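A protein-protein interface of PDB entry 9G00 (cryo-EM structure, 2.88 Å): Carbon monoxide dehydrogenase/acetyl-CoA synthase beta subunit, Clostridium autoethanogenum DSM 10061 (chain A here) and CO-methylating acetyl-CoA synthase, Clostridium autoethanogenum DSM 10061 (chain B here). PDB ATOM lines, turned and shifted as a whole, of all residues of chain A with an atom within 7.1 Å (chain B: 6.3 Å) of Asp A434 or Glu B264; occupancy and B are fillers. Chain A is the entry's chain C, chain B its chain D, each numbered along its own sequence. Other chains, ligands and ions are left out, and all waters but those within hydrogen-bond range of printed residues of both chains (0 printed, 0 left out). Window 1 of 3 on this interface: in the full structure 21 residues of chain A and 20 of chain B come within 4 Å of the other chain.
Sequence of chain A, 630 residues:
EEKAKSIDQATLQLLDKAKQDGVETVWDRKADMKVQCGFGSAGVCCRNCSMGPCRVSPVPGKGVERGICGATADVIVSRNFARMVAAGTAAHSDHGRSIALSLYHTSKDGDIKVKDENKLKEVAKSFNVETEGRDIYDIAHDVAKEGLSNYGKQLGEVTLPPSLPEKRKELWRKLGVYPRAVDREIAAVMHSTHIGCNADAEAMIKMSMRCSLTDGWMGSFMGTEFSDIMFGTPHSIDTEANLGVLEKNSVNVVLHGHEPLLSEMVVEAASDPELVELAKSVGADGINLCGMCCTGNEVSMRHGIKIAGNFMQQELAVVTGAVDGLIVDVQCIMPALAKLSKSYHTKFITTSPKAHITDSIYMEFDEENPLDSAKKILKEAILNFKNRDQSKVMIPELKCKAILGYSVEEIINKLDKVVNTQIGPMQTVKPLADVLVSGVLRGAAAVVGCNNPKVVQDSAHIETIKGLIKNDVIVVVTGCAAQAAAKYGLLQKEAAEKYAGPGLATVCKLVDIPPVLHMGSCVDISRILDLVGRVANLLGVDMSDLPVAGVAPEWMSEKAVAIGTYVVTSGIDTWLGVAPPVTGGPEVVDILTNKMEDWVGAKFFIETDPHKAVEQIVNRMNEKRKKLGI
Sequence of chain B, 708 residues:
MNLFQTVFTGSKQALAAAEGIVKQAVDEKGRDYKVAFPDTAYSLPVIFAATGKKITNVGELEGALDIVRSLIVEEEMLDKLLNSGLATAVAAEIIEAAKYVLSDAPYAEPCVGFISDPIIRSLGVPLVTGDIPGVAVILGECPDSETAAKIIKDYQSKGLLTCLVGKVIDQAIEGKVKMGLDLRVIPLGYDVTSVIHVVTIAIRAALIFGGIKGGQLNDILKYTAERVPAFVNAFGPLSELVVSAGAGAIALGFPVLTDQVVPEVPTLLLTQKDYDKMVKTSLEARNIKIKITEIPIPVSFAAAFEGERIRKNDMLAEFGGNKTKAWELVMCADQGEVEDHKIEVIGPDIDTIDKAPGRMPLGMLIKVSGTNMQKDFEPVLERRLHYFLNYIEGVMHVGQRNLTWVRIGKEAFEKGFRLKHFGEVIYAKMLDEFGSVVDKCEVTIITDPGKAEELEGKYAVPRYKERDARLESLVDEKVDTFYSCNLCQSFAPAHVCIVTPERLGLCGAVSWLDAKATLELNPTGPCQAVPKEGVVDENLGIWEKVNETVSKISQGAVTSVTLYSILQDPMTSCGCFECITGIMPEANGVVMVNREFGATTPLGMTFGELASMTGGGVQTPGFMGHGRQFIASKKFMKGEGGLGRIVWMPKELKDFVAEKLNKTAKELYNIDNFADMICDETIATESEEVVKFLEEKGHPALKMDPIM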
ATOM      1  N   ILE A 423     -32.880  36.970 -13.620  1.00  0.00           N
ATOM      2  CA  ILE A 423     -31.661  36.179 -13.781  1.00  0.00           C
ATOM      3  C   ILE A 423     -31.978  34.786 -14.319  1.00  0.00           C
ATOM      4  O   ILE A 423     -31.521  34.407 -15.398  1.00  0.00           O
ATOM      5  CB  ILE A 423     -30.864  36.104 -12.457  1.00  0.00           C
ATOM      6  CG1 ILE A 423     -30.493  37.514 -11.973  1.00  0.00           C
ATOM      7  CG2 ILE A 423     -29.611  35.234 -12.643  1.00  0.00           C
ATOM      8  CD1 ILE A 423     -29.901  37.535 -10.567  1.00  0.00           C
ATOM      9  N   GLY A 424     -32.754  34.005 -13.573  1.00  0.00           N
ATOM     10  CA  GLY A 424     -33.062  32.645 -13.934  1.00  0.00           C
ATOM     11  C   GLY A 424     -31.845  31.746 -13.830  1.00  0.00           C
ATOM     12  O   GLY A 424     -30.839  32.106 -13.216  1.00  0.00           O
ATOM     13  N   VAL A 429     -32.197  22.747 -10.475  1.00  0.00           N
ATOM     14  CA  VAL A 429     -31.753  22.530  -9.101  1.00  0.00           C
ATOM     15  C   VAL A 429     -30.708  23.589  -8.757  1.00  0.00           C
ATOM     16  O   VAL A 429     -30.033  23.516  -7.722  1.00  0.00           O
ATOM     17  CB  VAL A 429     -31.196  21.105  -8.923  1.00  0.00           C
ATOM     18  CG1 VAL A 429     -32.277  20.074  -9.264  1.00  0.00           C
ATOM     19  CG2 VAL A 429     -29.939  20.886  -9.793  1.00  0.00           C
ATOM     20  N   LYS A 430     -30.607  24.611  -9.607  1.00  0.00           N
ATOM     21  CA  LYS A 430     -29.560  25.609  -9.427  1.00  0.00           C
ATOM     22  C   LYS A 430     -29.596  26.313  -8.076  1.00  0.00           C
ATOM     23  O   LYS A 430     -28.513  26.537  -7.512  1.00  0.00           O
ATOM     24  CB  LYS A 430     -29.612  26.636 -10.558  1.00  0.00           C
ATOM     25  CG  LYS A 430     -28.433  27.602 -10.528  1.00  0.00           C
ATOM     26  CD  LYS A 430     -28.458  28.518 -11.744  1.00  0.00           C
ATOM     27  CE  LYS A 430     -27.172  29.341 -11.836  1.00  0.00           C
ATOM     28  NZ  LYS A 430     -26.986  30.202 -10.618  1.00  0.00           N
ATOM     29  N   PRO A 431     -30.745  26.725  -7.524  1.00  0.00           N
ATOM     30  CA  PRO A 431     -30.703  27.320  -6.170  1.00  0.00           C
ATOM     31  C   PRO A 431     -30.099  26.394  -5.115  1.00  0.00           C
ATOM     32  O   PRO A 431     -29.341  26.855  -4.251  1.00  0.00           O
ATOM     33  CB  PRO A 431     -32.174  27.668  -5.885  1.00  0.00           C
ATOM     34  CG  PRO A 431     -32.813  27.817  -7.256  1.00  0.00           C
ATOM     35  CD  PRO A 431     -32.079  26.822  -8.144  1.00  0.00           C
ATOM     36  N   LEU A 432     -30.403  25.096  -5.181  1.00  0.00           N
ATOM     37  CA  LEU A 432     -29.825  24.128  -4.252  1.00  0.00           C
ATOM     38  C   LEU A 432     -28.321  24.003  -4.458  1.00  0.00           C
ATOM     39  O   LEU A 432     -27.545  23.999  -3.492  1.00  0.00           O
ATOM     40  CB  LEU A 432     -30.511  22.765  -4.415  1.00  0.00           C
ATOM     41  CG  LEU A 432     -29.931  21.600  -3.590  1.00  0.00           C
ATOM     42  CD1 LEU A 432     -30.028  21.875  -2.075  1.00  0.00           C
ATOM     43  CD2 LEU A 432     -30.623  20.277  -3.957  1.00  0.00           C
ATOM     44  N   ALA A 433     -27.893  23.955  -5.715  1.00  0.00           N
ATOM     45  CA  ALA A 433     -26.467  23.923  -6.012  1.00  0.00           C
ATOM     46  C   ALA A 433     -25.788  25.181  -5.489  1.00  0.00           C
ATOM     47  O   ALA A 433     -24.674  25.119  -4.964  1.00  0.00           O
ATOM     48  CB  ALA A 433     -26.230  23.753  -7.513  1.00  0.00           C
ATOM     49  N   ASP A 434     -26.453  26.331  -5.600  1.00  0.00           N
ATOM     50  CA  ASP A 434     -25.880  27.589  -5.126  1.00  0.00           C
ATOM     51  C   ASP A 434     -25.710  27.590  -3.615  1.00  0.00           C
ATOM     52  O   ASP A 434     -24.647  27.959  -3.108  1.00  0.00           O
ATOM     53  CB  ASP A 434     -26.759  28.773  -5.536  1.00  0.00           C
ATOM     54  CG  ASP A 434     -26.776  29.013  -7.028  1.00  0.00           C
ATOM     55  OD1 ASP A 434     -25.745  28.732  -7.677  1.00  0.00           O
ATOM     56  OD2 ASP A 434     -27.803  29.481  -7.555  1.00  0.00           O
ATOM     57  N   VAL A 435     -26.729  27.159  -2.874  1.00  0.00           N
ATOM     58  CA  VAL A 435     -26.598  27.173  -1.412  1.00  0.00           C
ATOM     59  C   VAL A 435     -25.532  26.173  -0.958  1.00  0.00           C
ATOM     60  O   VAL A 435     -24.711  26.476  -0.061  1.00  0.00           O
ATOM     61  CB  VAL A 435     -27.961  26.924  -0.728  1.00  0.00           C
ATOM     62  CG1 VAL A 435     -28.976  28.005  -1.124  1.00  0.00           C
ATOM     63  CG2 VAL A 435     -28.509  25.543  -1.043  1.00  0.00           C
ATOM     64  N   LEU A 436     -25.416  25.040  -1.665  1.00  0.00           N
ATOM     65  CA  LEU A 436     -24.371  24.075  -1.327  1.00  0.00           C
ATOM     66  C   LEU A 436     -22.984  24.621  -1.650  1.00  0.00           C
ATOM     67  O   LEU A 436     -22.060  24.476  -0.845  1.00  0.00           O
ATOM     68  CB  LEU A 436     -24.600  22.753  -2.069  1.00  0.00           C
ATOM     69  CG  LEU A 436     -25.771  21.904  -1.549  1.00  0.00           C
ATOM     70  CD1 LEU A 436     -25.989  20.697  -2.462  1.00  0.00           C
ATOM     71  CD2 LEU A 436     -25.563  21.460  -0.080  1.00  0.00           C
ATOM     72  N   VAL A 437     -22.817  25.257  -2.810  1.00  0.00           N
ATOM     73  CA  VAL A 437     -21.496  25.745  -3.190  1.00  0.00           C
ATOM     74  C   VAL A 437     -21.081  26.901  -2.288  1.00  0.00           C
ATOM     75  O   VAL A 437     -19.921  26.996  -1.875  1.00  0.00           O
ATOM     76  CB  VAL A 437     -21.491  26.145  -4.678  1.00  0.00           C
ATOM     77  CG1 VAL A 437     -20.300  27.064  -5.009  1.00  0.00           C
ATOM     78  CG2 VAL A 437     -21.479  24.889  -5.568  1.00  0.00           C
ATOM     79  N   SER A 438     -22.007  27.818  -1.986  1.00  0.00           N
ATOM     80  CA  SER A 438     -21.646  28.964  -1.159  1.00  0.00           C
ATOM     81  C   SER A 438     -21.297  28.551   0.265  1.00  0.00           C
ATOM     82  O   SER A 438     -20.573  29.287   0.943  1.00  0.00           O
ATOM     83  CB  SER A 438     -22.772  30.014  -1.153  1.00  0.00           C
ATOM     84  OG  SER A 438     -23.910  29.548  -0.437  1.00  0.00           O
ATOM     85  N   GLY A 439     -21.749  27.376   0.718  1.00  0.00           N
ATOM     86  CA  GLY A 439     -21.490  26.979   2.086  1.00  0.00           C
ATOM     87  C   GLY A 439     -22.564  27.358   3.077  1.00  0.00           C
ATOM     88  O   GLY A 439     -22.415  27.060   4.267  1.00  0.00           O
ATOM     89  N   VAL A 440     -23.640  28.005   2.627  1.00  0.00           N
ATOM     90  CA  VAL A 440     -24.772  28.270   3.507  1.00  0.00           C
ATOM     91  C   VAL A 440     -25.331  26.947   4.011  1.00  0.00           C
ATOM     92  O   VAL A 440     -25.691  26.807   5.186  1.00  0.00           O
ATOM     93  CB  VAL A 440     -25.833  29.124   2.792  1.00  0.00           C
ATOM     94  CG1 VAL A 440     -27.105  29.248   3.636  1.00  0.00           C
ATOM     95  CG2 VAL A 440     -25.268  30.524   2.483  1.00  0.00           C
ATOM     96  N   LEU A 441     -25.427  25.962   3.124  1.00  0.00           N
ATOM     97  CA  LEU A 441     -25.664  24.574   3.497  1.00  0.00           C
ATOM     98  C   LEU A 441     -24.344  23.818   3.380  1.00  0.00           C
ATOM     99  O   LEU A 441     -23.648  23.918   2.363  1.00  0.00           O
ATOM    100  CB  LEU A 441     -26.739  23.923   2.622  1.00  0.00           C
ATOM    101  CG  LEU A 441     -28.182  24.408   2.836  1.00  0.00           C
ATOM    102  CD1 LEU A 441     -29.115  23.517   2.009  1.00  0.00           C
ATOM    103  CD2 LEU A 441     -28.623  24.442   4.310  1.00  0.00           C
ATOM    104  N   VAL A 535     -27.636  17.732  -9.484  1.00  0.00           N
ATOM    105  CA  VAL A 535     -26.700  18.690  -8.901  1.00  0.00           C
ATOM    106  C   VAL A 535     -25.317  18.504  -9.509  1.00  0.00           C
ATOM    107  O   VAL A 535     -24.669  19.459  -9.959  1.00  0.00           O
ATOM    108  CB  VAL A 535     -26.677  18.549  -7.372  1.00  0.00           C
ATOM    109  CG1 VAL A 535     -25.601  19.447  -6.766  1.00  0.00           C
ATOM    110  CG2 VAL A 535     -28.048  18.883  -6.805  1.00  0.00           C
ATOM    111  N   LEU A 538     -25.139  19.777 -12.920  1.00  0.00           N
ATOM    112  CA  LEU A 538     -25.147  21.228 -12.990  1.00  0.00           C
ATOM    113  C   LEU A 538     -23.785  21.804 -12.664  1.00  0.00           C
ATOM    114  O   LEU A 538     -23.413  22.847 -13.205  1.00  0.00           O
ATOM    115  CB  LEU A 538     -26.220  21.803 -12.055  1.00  0.00           C
ATOM    116  CG  LEU A 538     -26.596  23.274 -12.304  1.00  0.00           C
ATOM    117  CD1 LEU A 538     -26.697  23.612 -13.797  1.00  0.00           C
ATOM    118  CD2 LEU A 538     -27.917  23.586 -11.627  1.00  0.00           C
ATOM    119  N   LEU A 539     -23.006  21.101 -11.845  1.00  0.00           N
ATOM    120  CA  LEU A 539     -21.698  21.582 -11.424  1.00  0.00           C
ATOM    121  C   LEU A 539     -20.561  21.003 -12.256  1.00  0.00           C
ATOM    122  O   LEU A 539     -19.404  21.381 -12.047  1.00  0.00           O
ATOM    123  CB  LEU A 539     -21.467  21.267  -9.939  1.00  0.00           C
ATOM    124  CG  LEU A 539     -22.405  21.989  -8.957  1.00  0.00           C
ATOM    125  CD1 LEU A 539     -22.122  21.541  -7.533  1.00  0.00           C
ATOM    126  CD2 LEU A 539     -22.286  23.521  -9.081  1.00  0.00           C
ATOM    127  N   LEU B   3     -16.494  31.319  -0.309  1.00  0.00           N
ATOM    128  CA  LEU B   3     -17.163  32.534   0.151  1.00  0.00           C
ATOM    129  C   LEU B   3     -16.807  32.871   1.594  1.00  0.00           C
ATOM    130  O   LEU B   3     -16.462  34.021   1.910  1.00  0.00           O
ATOM    131  CB  LEU B   3     -18.681  32.374   0.003  1.00  0.00           C
ATOM    132  CG  LEU B   3     -19.517  33.564   0.503  1.00  0.00           C
ATOM    133  CD1 LEU B   3     -19.194  34.819  -0.312  1.00  0.00           C
ATOM    134  CD2 LEU B   3     -21.017  33.250   0.459  1.00  0.00           C
ATOM    135  N   VAL B 262     -19.540  35.195  -8.565  1.00  0.00           N
ATOM    136  CA  VAL B 262     -19.411  35.011  -7.118  1.00  0.00           C
ATOM    137  C   VAL B 262     -20.160  33.756  -6.712  1.00  0.00           C
ATOM    138  O   VAL B 262     -20.993  33.233  -7.466  1.00  0.00           O
ATOM    139  CB  VAL B 262     -19.952  36.223  -6.331  1.00  0.00           C
ATOM    140  CG1 VAL B 262     -19.158  37.486  -6.662  1.00  0.00           C
ATOM    141  CG2 VAL B 262     -21.439  36.427  -6.614  1.00  0.00           C
ATOM    142  N   PRO B 263     -19.871  33.231  -5.507  1.00  0.00           N
ATOM    143  CA  PRO B 263     -20.682  32.124  -4.969  1.00  0.00           C
ATOM    144  C   PRO B 263     -22.063  32.603  -4.561  1.00  0.00           C
ATOM    145  O   PRO B 263     -22.315  32.967  -3.406  1.00  0.00           O
ATOM    146  CB  PRO B 263     -19.869  31.621  -3.768  1.00  0.00           C
ATOM    147  CG  PRO B 263     -18.453  32.097  -4.029  1.00  0.00           C
ATOM    148  CD  PRO B 263     -18.615  33.414  -4.755  1.00  0.00           C
ATOM    149  N   GLU B 264     -22.969  32.599  -5.532  1.00  0.00           N
ATOM    150  CA  GLU B 264     -24.296  33.157  -5.343  1.00  0.00           C
ATOM    151  C   GLU B 264     -25.045  32.491  -4.192  1.00  0.00           C
ATOM    152  O   GLU B 264     -24.973  31.273  -3.996  1.00  0.00           O
ATOM    153  CB  GLU B 264     -25.104  33.016  -6.628  1.00  0.00           C
ATOM    154  CG  GLU B 264     -24.784  34.080  -7.668  1.00  0.00           C
ATOM    155  CD  GLU B 264     -25.661  33.923  -8.889  1.00  0.00           C
ATOM    156  OE1 GLU B 264     -25.582  32.860  -9.530  1.00  0.00           O
ATOM    157  OE2 GLU B 264     -26.450  34.842  -9.188  1.00  0.00           O
ATOM    158  N   VAL B 265     -25.752  33.314  -3.428  1.00  0.00           N
ATOM    159  CA  VAL B 265     -26.674  32.882  -2.389  1.00  0.00           C
ATOM    160  C   VAL B 265     -28.066  33.386  -2.763  1.00  0.00           C
ATOM    161  O   VAL B 265     -28.265  34.599  -2.881  1.00  0.00           O
ATOM    162  CB  VAL B 265     -26.256  33.414  -1.007  1.00  0.00           C
ATOM    163  CG1 VAL B 265     -27.257  32.975   0.061  1.00  0.00           C
ATOM    164  CG2 VAL B 265     -24.824  32.961  -0.671  1.00  0.00           C
ATOM    165  N   PRO B 266     -29.072  32.516  -2.908  1.00  0.00           N
ATOM    166  CA  PRO B 266     -30.390  32.991  -3.368  1.00  0.00           C
ATOM    167  C   PRO B 266     -30.940  34.099  -2.476  1.00  0.00           C
ATOM    168  O   PRO B 266     -30.842  34.056  -1.248  1.00  0.00           O
ATOM    169  CB  PRO B 266     -31.262  31.730  -3.327  1.00  0.00           C
ATOM    170  CG  PRO B 266     -30.286  30.588  -3.532  1.00  0.00           C
ATOM    171  CD  PRO B 266     -29.013  31.044  -2.822  1.00  0.00           C
ATOM    172  N   LEU B 269     -27.048  37.154  -2.472  1.00  0.00           N
ATOM    173  CA  LEU B 269     -25.876  37.483  -3.275  1.00  0.00           C
ATOM    174  C   LEU B 269     -26.141  36.956  -4.678  1.00  0.00           C
ATOM    175  O   LEU B 269     -26.260  35.743  -4.876  1.00  0.00           O
ATOM    176  CB  LEU B 269     -24.616  36.875  -2.660  1.00  0.00           C
ATOM    177  CG  LEU B 269     -23.298  37.190  -3.367  1.00  0.00           C
ATOM    178  CD1 LEU B 269     -23.050  38.690  -3.433  1.00  0.00           C
ATOM    179  CD2 LEU B 269     -22.164  36.478  -2.642  1.00  0.00           C
ATOM    180  N   LEU B 270     -26.261  37.867  -5.640  1.00  0.00           N
ATOM    181  CA  LEU B 270     -26.690  37.528  -6.989  1.00  0.00           C
ATOM    182  C   LEU B 270     -25.762  38.140  -8.027  1.00  0.00           C
ATOM    183  O   LEU B 270     -25.303  39.275  -7.876  1.00  0.00           O
ATOM    184  CB  LEU B 270     -28.124  38.005  -7.251  1.00  0.00           C
ATOM    185  CG  LEU B 270     -29.197  37.574  -6.240  1.00  0.00           C
ATOM    186  CD1 LEU B 270     -30.519  38.270  -6.567  1.00  0.00           C
ATOM    187  CD2 LEU B 270     -29.366  36.055  -6.217  1.00  0.00           C
ATOM    188  N   THR B 271     -25.532  37.395  -9.102  1.00  0.00           N
ATOM    189  CA  THR B 271     -24.727  37.853 -10.222  1.00  0.00           C
ATOM    190  C   THR B 271     -25.651  38.207 -11.377  1.00  0.00           C
ATOM    191  O   THR B 271     -26.500  37.399 -11.768  1.00  0.00           O
ATOM    192  CB  THR B 271     -23.728  36.780 -10.677  1.00  0.00           C
ATOM    193  OG1 THR B 271     -22.698  36.599  -9.695  1.00  0.00           O
ATOM    194  CG2 THR B 271     -23.082  37.173 -12.012  1.00  0.00           C
ATOM    195  N   GLN B 272     -25.491  39.418 -11.909  1.00  0.00           N
ATOM    196  CA  GLN B 272     -26.246  39.879 -13.070  1.00  0.00           C
ATOM    197  C   GLN B 272     -25.240  40.603 -13.961  1.00  0.00           C
ATOM    198  O   GLN B 272     -24.841  41.733 -13.662  1.00  0.00           O
ATOM    199  CB  GLN B 272     -27.404  40.792 -12.661  1.00  0.00           C
ATOM    200  CG  GLN B 272     -28.165  41.401 -13.851  1.00  0.00           C
ATOM    201  CD  GLN B 272     -28.748  40.321 -14.761  1.00  0.00           C
ATOM    202  OE1 GLN B 272     -28.137  39.947 -15.751  1.00  0.00           O
ATOM    203  NE2 GLN B 272     -29.930  39.807 -14.412  1.00  0.00           N
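The side-chain amino group (NZ) of Lys A430 lies within salt-bridge range of the side-chain carboxylate (OD2) of Asp A434 (3.3 Å). The backbone carbonyl oxygen of Val A435 sits at hydrogen-bond distance from the backbone NH of Leu A441 (3.3 Å). The backbone carbonyl oxygen (O) of Val A435 is in hydrogen-bond range of the backbone NH (N) of Val A440 (3.3 Å). The side-chain hydroxyl of Ser A438 lies within hydrogen-bond range of the backbone carbonyl oxygen of Val A435, 3.2 Å away. The side-chain hydroxyl of Ser A438 lies close to the backbone NH of Val A440 (3.4 Å). OE2 of Glu B264 lies within hydrogen-bond range of N of Thr B271 (2.7 Å).
The backbone carbonyl oxygen of Asp A434 lies close to the backbone carbonyl oxygen of Glu B264 (3.4 Å). The side-chain carboxylate (OE1) of Glu B264 lies within salt-bridge range of the side-chain amino group (NZ) of Lys A430 (3.2 Å).
Among the printed residues, merely in contact across the chains: Ile A423 with Leu B270, Ile A423 with Thr B271, Ile A423 with Gln B272, Pro A431 with Pro B266, Val A435 with Pro B266, Ser A438 with Leu B3, Ser A438 with Pro B263, Ser A438 with Glu B264, Ser A438 with Val B265 and Val A440 with Val B265.
Asp A434 touches just one residue of chain B: Glu B264 (3.4 Å). Of chain A, only Lys A430 (3.2 Å), Asp A434 (3.4 Å) and Ser A438 (3.8 Å) come within 4 Å of Glu B264. Of the printed residues of chain B, Pro A431 touches Pro B266 (3.9 Å). Printed residues of chain A within 4 Å of Thr B271: Ile A423. The nearest printed residue of chain A that does not touch Glu B264 is Ile A423 (4.6 Å). The nearest printed residue of chain B that does not touch Ser A438 is Pro B266 (5.8 Å).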
